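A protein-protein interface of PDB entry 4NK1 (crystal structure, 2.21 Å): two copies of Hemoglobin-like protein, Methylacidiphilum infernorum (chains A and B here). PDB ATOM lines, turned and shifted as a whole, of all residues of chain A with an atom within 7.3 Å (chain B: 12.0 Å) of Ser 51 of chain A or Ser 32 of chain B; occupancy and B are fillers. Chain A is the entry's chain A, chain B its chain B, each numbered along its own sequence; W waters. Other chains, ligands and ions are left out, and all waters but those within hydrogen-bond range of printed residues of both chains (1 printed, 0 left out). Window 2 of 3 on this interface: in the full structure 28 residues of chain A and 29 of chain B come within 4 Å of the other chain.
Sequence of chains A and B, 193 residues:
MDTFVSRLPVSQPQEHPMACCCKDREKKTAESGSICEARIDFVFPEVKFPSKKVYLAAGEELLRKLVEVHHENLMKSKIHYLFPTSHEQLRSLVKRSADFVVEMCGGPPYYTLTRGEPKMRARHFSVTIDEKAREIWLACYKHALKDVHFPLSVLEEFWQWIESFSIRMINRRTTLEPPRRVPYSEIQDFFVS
The backbone NH (N) of Phe 49 of chain A is in hydrogen-bond range of the backbone carbonyl oxygen (O) of Ser 34 of chain B.
NZ of Lys 48 of chain A lies within salt-bridge range of OE1 of Glu 157 of chain A (3.5 Å).
The side-chain hydroxyl (OG) of Ser 51 of chain A is in hydrogen-bond range of the side-chain amino group (NZ) of Lys 53 of chain A (2.9 Å).
The side-chain carboxylate (OE1) of Glu 157 of chain A lies within hydrogen-bond range of the backbone NH (N) of Ser 51 of chain A (2.6 Å).
Gly 33 of chain B touches Lys 48 of chain A.
Lys 48 of chain A touches Ser 34 of chain B.
CG of Lys 48 of chain A touches CG1 of Ile 35 of chain B (3.6 Å).
O of Phe 49 of chain A touches CA of Gly 33 of chain B (3.6 Å).
SG of Cys 36 of chain B touches CE1 of Phe 49 of chain A (3.7 Å).
O of Pro 50 of chain A touches CA of Gly 33 of chain B, at 3.9 Å.
Ser 51 of chain A touches Ser 32 of chain B (CB to CB, 3.5 Å).
Ser 51 of chain A touches Gly 33 of chain B (CB to N, 3.9 Å).
Of the printed residues of chain B, Ser 51 of chain A touches Ser 32 and Gly 33.
Of the printed residues of chain A, Ser 32 of chain B touches Ser 51 (3.5 Å).
Of chain B, only Gly 33 comes within 4 Å of Pro 50 of chain A.
No residue of chain B comes within 4 Å of Val 54 of chain A.
No residue of chain B comes within 4 Å of Cys 105 of chain A.
Gly 106 of chain A touches none of the printed residues of chain B.
Of the printed residues of chain A, Gly 33 of chain B touches Lys 48 (3.8 Å), Phe 49 (3.6 Å), Pro 50 (3.9 Å) and Ser 51 (3.9 Å).
Of the printed residues of chain B, Phe 49 of chain A touches Gly 33 (3.6 Å), Ser 34 (2.8 Å) and Cys 36 (3.7 Å).
Of the printed residues of chain B, Lys 48 of chain A touches Gly 33, Ser 34 and Ile 35.
Met 104 of chain A touches none of the printed residues of chain B.
Val 154 of chain A touches none of the printed residues of chain B.
The nearest residue of chain B that does not touch Ser 51 of chain A is Ser 34 of chain B (6.0 Å).
The nearest residue of chain A that does not touch Ser 32 of chain B is Lys 53 of chain A (4.3 Å).
Of the 16 printed residues of chain A, 4 touch a printed residue of chain B.
Printed residues of chain A that touch a printed residue of chain B: Lys 48, Phe 49, Pro 50 and Ser 51.
Hydrophobic or aromatic side chains of chain A within 4 Å of the printed part of chain B: Phe 49.
Among the printed residues, 9 pairs touch across the chains.
Among the printed residues, no Asp or Glu carboxylate lies within 4 Å of a Lys or Arg side-chain nitrogen of the other chain.
No position is printed for both chains.
Water W1 lies within hydrogen-bond range of O of Ser 32 of chain B and N of Lys 52 of chain A.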
ATOM      1  N   LYS A  48     -17.457  -1.331   5.625  1.00  0.00           N
ATOM      2  CA  LYS A  48     -16.921  -2.173   6.681  1.00  0.00           C
ATOM      3  C   LYS A  48     -15.668  -2.877   6.168  1.00  0.00           C
ATOM      4  O   LYS A  48     -15.740  -3.715   5.269  1.00  0.00           O
ATOM      5  CB  LYS A  48     -17.968  -3.182   7.150  1.00  0.00           C
ATOM      6  CG  LYS A  48     -17.926  -3.478   8.656  1.00  0.00           C
ATOM      7  CD  LYS A  48     -16.763  -4.402   9.054  1.00  0.00           C
ATOM      8  CE  LYS A  48     -17.227  -5.850   9.283  1.00  0.00           C
ATOM      9  NZ  LYS A  48     -16.082  -6.813   9.443  1.00  0.00           N
ATOM     10  N   PHE A  49     -14.519  -2.510   6.720  1.00  0.00           N
ATOM     11  CA  PHE A  49     -13.282  -3.182   6.375  1.00  0.00           C
ATOM     12  C   PHE A  49     -13.287  -4.575   6.983  1.00  0.00           C
ATOM     13  O   PHE A  49     -13.863  -4.787   8.050  1.00  0.00           O
ATOM     14  CB  PHE A  49     -12.081  -2.381   6.871  1.00  0.00           C
ATOM     15  CG  PHE A  49     -11.644  -1.292   5.915  1.00  0.00           C
ATOM     16  CD1 PHE A  49     -12.445  -0.172   5.695  1.00  0.00           C
ATOM     17  CD2 PHE A  49     -10.429  -1.390   5.240  1.00  0.00           C
ATOM     18  CE1 PHE A  49     -12.041   0.841   4.812  1.00  0.00           C
ATOM     19  CE2 PHE A  49     -10.015  -0.387   4.354  1.00  0.00           C
ATOM     20  CZ  PHE A  49     -10.824   0.730   4.142  1.00  0.00           C
ATOM     21  N   PRO A  50     -12.638  -5.529   6.304  1.00  0.00           N
ATOM     22  CA  PRO A  50     -12.672  -6.929   6.739  1.00  0.00           C
ATOM     23  C   PRO A  50     -11.983  -7.104   8.086  1.00  0.00           C
ATOM     24  O   PRO A  50     -11.044  -6.360   8.382  1.00  0.00           O
ATOM     25  CB  PRO A  50     -11.841  -7.648   5.668  1.00  0.00           C
ATOM     26  CG  PRO A  50     -11.772  -6.700   4.501  1.00  0.00           C
ATOM     27  CD  PRO A  50     -11.793  -5.330   5.110  1.00  0.00           C
ATOM     28  N   SER A  51     -12.438  -8.062   8.888  1.00  0.00           N
ATOM     29  CA  SER A  51     -11.725  -8.434  10.105  1.00  0.00           C
ATOM     30  C   SER A  51     -10.522  -9.301   9.746  1.00  0.00           C
ATOM     31  O   SER A  51     -10.395  -9.739   8.611  1.00  0.00           O
ATOM     32  CB  SER A  51     -12.642  -9.199  11.049  1.00  0.00           C
ATOM     33  OG  SER A  51     -13.180 -10.357  10.425  1.00  0.00           O
ATOM     34  N   LYS A  52      -9.644  -9.548  10.716  1.00  0.00           N
ATOM     35  CA  LYS A  52      -8.482 -10.413  10.516  1.00  0.00           C
ATOM     36  C   LYS A  52      -8.870 -11.864  10.146  1.00  0.00           C
ATOM     37  O   LYS A  52      -8.047 -12.611   9.597  1.00  0.00           O
ATOM     38  CB  LYS A  52      -7.606 -10.384  11.779  1.00  0.00           C
ATOM     39  CG  LYS A  52      -6.250 -11.065  11.662  1.00  0.00           C
ATOM     40  CD  LYS A  52      -5.280 -10.466  12.679  1.00  0.00           C
ATOM     41  CE  LYS A  52      -4.256 -11.475  13.183  1.00  0.00           C
ATOM     42  NZ  LYS A  52      -3.344 -11.950  12.118  1.00  0.00           N
ATOM     43  N   LYS A  53     -10.117 -12.247  10.428  1.00  0.00           N
ATOM     44  CA  LYS A  53     -10.658 -13.543   9.979  1.00  0.00           C
ATOM     45  C   LYS A  53     -10.441 -13.816   8.486  1.00  0.00           C
ATOM     46  O   LYS A  53     -10.179 -14.957   8.094  1.00  0.00           O
ATOM     47  CB  LYS A  53     -12.161 -13.650  10.284  1.00  0.00           C
ATOM     48  CG  LYS A  53     -12.505 -13.962  11.744  1.00  0.00           C
ATOM     49  CD  LYS A  53     -14.008 -13.784  12.005  1.00  0.00           C
ATOM     50  CE  LYS A  53     -14.328 -12.378  12.542  1.00  0.00           C
ATOM     51  NZ  LYS A  53     -15.400 -11.668  11.762  1.00  0.00           N
ATOM     52  N   VAL A  54     -10.574 -12.790   7.648  1.00  0.00           N
ATOM     53  CA  VAL A  54     -10.353 -12.982   6.214  1.00  0.00           C
ATOM     54  C   VAL A  54      -8.925 -13.447   5.933  1.00  0.00           C
ATOM     55  O   VAL A  54      -8.710 -14.391   5.170  1.00  0.00           O
ATOM     56  CB  VAL A  54     -10.663 -11.708   5.400  1.00  0.00           C
ATOM     57  CG1 VAL A  54     -10.403 -11.937   3.913  1.00  0.00           C
ATOM     58  CG2 VAL A  54     -12.107 -11.279   5.633  1.00  0.00           C
ATOM     59  N   TYR A  55      -7.947 -12.809   6.564  1.00  0.00           N
ATOM     60  CA  TYR A  55      -6.549 -13.201   6.372  1.00  0.00           C
ATOM     61  C   TYR A  55      -6.230 -14.578   6.986  1.00  0.00           C
ATOM     62  O   TYR A  55      -5.495 -15.377   6.405  1.00  0.00           O
ATOM     63  CB  TYR A  55      -5.621 -12.115   6.935  1.00  0.00           C
ATOM     64  CG  TYR A  55      -4.182 -12.540   7.094  1.00  0.00           C
ATOM     65  CD1 TYR A  55      -3.312 -12.548   6.009  1.00  0.00           C
ATOM     66  CD2 TYR A  55      -3.686 -12.924   8.336  1.00  0.00           C
ATOM     67  CE1 TYR A  55      -1.983 -12.926   6.156  1.00  0.00           C
ATOM     68  CE2 TYR A  55      -2.350 -13.308   8.494  1.00  0.00           C
ATOM     69  CZ  TYR A  55      -1.514 -13.309   7.403  1.00  0.00           C
ATOM     70  OH  TYR A  55      -0.203 -13.691   7.568  1.00  0.00           O
ATOM     71  N   LEU A  56      -6.766 -14.850   8.168  1.00  0.00           N
ATOM     72  CA  LEU A  56      -6.559 -16.156   8.801  1.00  0.00           C
ATOM     73  C   LEU A  56      -7.219 -17.266   7.985  1.00  0.00           C
ATOM     74  O   LEU A  56      -6.687 -18.370   7.873  1.00  0.00           O
ATOM     75  CB  LEU A  56      -7.147 -16.155  10.209  1.00  0.00           C
ATOM     76  CG  LEU A  56      -6.583 -15.121  11.175  1.00  0.00           C
ATOM     77  CD1 LEU A  56      -7.379 -15.131  12.482  1.00  0.00           C
ATOM     78  CD2 LEU A  56      -5.120 -15.416  11.435  1.00  0.00           C
ATOM     79  N   MET A 104      -5.113  -5.008   4.534  1.00  0.00           N
ATOM     80  CA  MET A 104      -6.482  -4.619   4.886  1.00  0.00           C
ATOM     81  C   MET A 104      -7.333  -5.776   5.376  1.00  0.00           C
ATOM     82  O   MET A 104      -8.316  -5.567   6.088  1.00  0.00           O
ATOM     83  CB  MET A 104      -7.182  -3.943   3.705  1.00  0.00           C
ATOM     84  CG  MET A 104      -6.585  -2.610   3.309  1.00  0.00           C
ATOM     85  SD  MET A 104      -6.644  -1.379   4.632  1.00  0.00           S
ATOM     86  CE  MET A 104      -4.969  -1.432   5.226  1.00  0.00           C
ATOM     87  N   CYS A 105      -6.957  -6.996   4.999  1.00  0.00           N
ATOM     88  CA  CYS A 105      -7.659  -8.185   5.489  1.00  0.00           C
ATOM     89  C   CYS A 105      -7.101  -8.684   6.819  1.00  0.00           C
ATOM     90  O   CYS A 105      -7.604  -9.656   7.379  1.00  0.00           O
ATOM     91  CB  CYS A 105      -7.635  -9.302   4.446  1.00  0.00           C
ATOM     92  SG  CYS A 105      -8.672  -8.919   3.000  1.00  0.00           S
ATOM     93  N   GLY A 106      -6.072  -8.010   7.331  1.00  0.00           N
ATOM     94  CA  GLY A 106      -5.544  -8.327   8.647  1.00  0.00           C
ATOM     95  C   GLY A 106      -4.166  -8.967   8.630  1.00  0.00           C
ATOM     96  O   GLY A 106      -3.689  -9.444   9.658  1.00  0.00           O
ATOM     97  N   GLY A 107      -3.514  -8.982   7.473  1.00  0.00           N
ATOM     98  CA  GLY A 107      -2.163  -9.513   7.406  1.00  0.00           C
ATOM     99  C   GLY A 107      -1.120  -8.454   7.727  1.00  0.00           C
ATOM    100  O   GLY A 107      -1.455  -7.369   8.233  1.00  0.00           O
ATOM    101  N   VAL A 154     -15.722 -16.394   4.536  1.00  0.00           N
ATOM    102  CA  VAL A 154     -15.318 -14.993   4.615  1.00  0.00           C
ATOM    103  C   VAL A 154     -15.554 -14.252   3.297  1.00  0.00           C
ATOM    104  O   VAL A 154     -15.198 -13.082   3.160  1.00  0.00           O
ATOM    105  CB  VAL A 154     -13.846 -14.860   5.040  1.00  0.00           C
ATOM    106  CG1 VAL A 154     -13.668 -15.336   6.459  1.00  0.00           C
ATOM    107  CG2 VAL A 154     -12.963 -15.649   4.097  1.00  0.00           C
ATOM    108  N   GLU A 157     -17.794 -11.128   3.692  1.00  0.00           N
ATOM    109  CA  GLU A 157     -16.995 -10.119   4.387  1.00  0.00           C
ATOM    110  C   GLU A 157     -16.082  -9.366   3.415  1.00  0.00           C
ATOM    111  O   GLU A 157     -16.063  -8.128   3.396  1.00  0.00           O
ATOM    112  CB  GLU A 157     -16.185 -10.763   5.517  1.00  0.00           C
ATOM    113  CG  GLU A 157     -15.619  -9.745   6.491  1.00  0.00           C
ATOM    114  CD  GLU A 157     -15.145 -10.358   7.800  1.00  0.00           C
ATOM    115  OE1 GLU A 157     -14.371  -9.680   8.502  1.00  0.00           O
ATOM    116  OE2 GLU A 157     -15.553 -11.499   8.139  1.00  0.00           O
ATOM    117  N   PHE A 158     -15.362 -10.104   2.574  1.00  0.00           N
ATOM    118  CA  PHE A 158     -14.527  -9.473   1.560  1.00  0.00           C
ATOM    119  C   PHE A 158     -15.373  -8.714   0.533  1.00  0.00           C
ATOM    120  O   PHE A 158     -15.039  -7.588   0.155  1.00  0.00           O
ATOM    121  CB  PHE A 158     -13.653 -10.503   0.850  1.00  0.00           C
ATOM    122  CG  PHE A 158     -12.669  -9.888  -0.113  1.00  0.00           C
ATOM    123  CD1 PHE A 158     -13.019  -9.642  -1.430  1.00  0.00           C
ATOM    124  CD2 PHE A 158     -11.397  -9.537   0.311  1.00  0.00           C
ATOM    125  CE1 PHE A 158     -12.109  -9.065  -2.315  1.00  0.00           C
ATOM    126  CE2 PHE A 158     -10.495  -8.956  -0.566  1.00  0.00           C
ATOM    127  CZ  PHE A 158     -10.856  -8.723  -1.883  1.00  0.00           C
ATOM    128  N   SER B  32     -14.762  -6.078  14.998  1.00  0.00           N
ATOM    129  CA  SER B  32     -13.524  -6.779  14.667  1.00  0.00           C
ATOM    130  C   SER B  32     -12.727  -6.010  13.614  1.00  0.00           C
ATOM    131  O   SER B  32     -11.529  -5.773  13.785  1.00  0.00           O
ATOM    132  CB  SER B  32     -13.818  -8.203  14.182  1.00  0.00           C
ATOM    133  OG  SER B  32     -14.622  -8.917  15.107  1.00  0.00           O
ATOM    134  N   GLY B  33     -13.398  -5.621  12.529  1.00  0.00           N
ATOM    135  CA  GLY B  33     -12.768  -4.827  11.482  1.00  0.00           C
ATOM    136  C   GLY B  33     -13.248  -3.381  11.458  1.00  0.00           C
ATOM    137  O   GLY B  33     -14.399  -3.090  11.794  1.00  0.00           O
ATOM    138  N   SER B  34     -12.365  -2.475  11.051  1.00  0.00           N
ATOM    139  CA  SER B  34     -12.656  -1.039  11.067  1.00  0.00           C
ATOM    140  C   SER B  34     -13.887  -0.646  10.241  1.00  0.00           C
ATOM    141  O   SER B  34     -14.228  -1.309   9.255  1.00  0.00           O
ATOM    142  CB  SER B  34     -11.430  -0.255  10.598  1.00  0.00           C
ATOM    143  OG  SER B  34     -11.792   1.033  10.132  1.00  0.00           O
ATOM    144  N   ILE B  35     -14.557   0.426  10.658  1.00  0.00           N
ATOM    145  CA  ILE B  35     -15.755   0.903   9.967  1.00  0.00           C
ATOM    146  C   ILE B  35     -15.663   2.388   9.617  1.00  0.00           C
ATOM    147  O   ILE B  35     -15.457   3.230  10.494  1.00  0.00           O
ATOM    148  CB  ILE B  35     -17.015   0.682  10.814  1.00  0.00           C
ATOM    149  CG1 ILE B  35     -17.267  -0.815  11.000  1.00  0.00           C
ATOM    150  CG2 ILE B  35     -18.217   1.362  10.167  1.00  0.00           C
ATOM    151  CD1 ILE B  35     -18.643  -1.143  11.548  1.00  0.00           C
ATOM    152  N   CYS B  36     -15.811   2.712   8.337  1.00  0.00           N
ATOM    153  CA  CYS B  36     -15.811   4.108   7.919  1.00  0.00           C
ATOM    154  C   CYS B  36     -17.245   4.587   7.779  1.00  0.00           C
ATOM    155  O   CYS B  36     -18.051   3.968   7.077  1.00  0.00           O
ATOM    156  CB  CYS B  36     -15.055   4.282   6.604  1.00  0.00           C
ATOM    157  SG  CYS B  36     -13.319   3.778   6.706  1.00  0.00           S
HETATM  158  O   HOH W   1     -10.209  -8.026  13.567  1.00  0.00           O
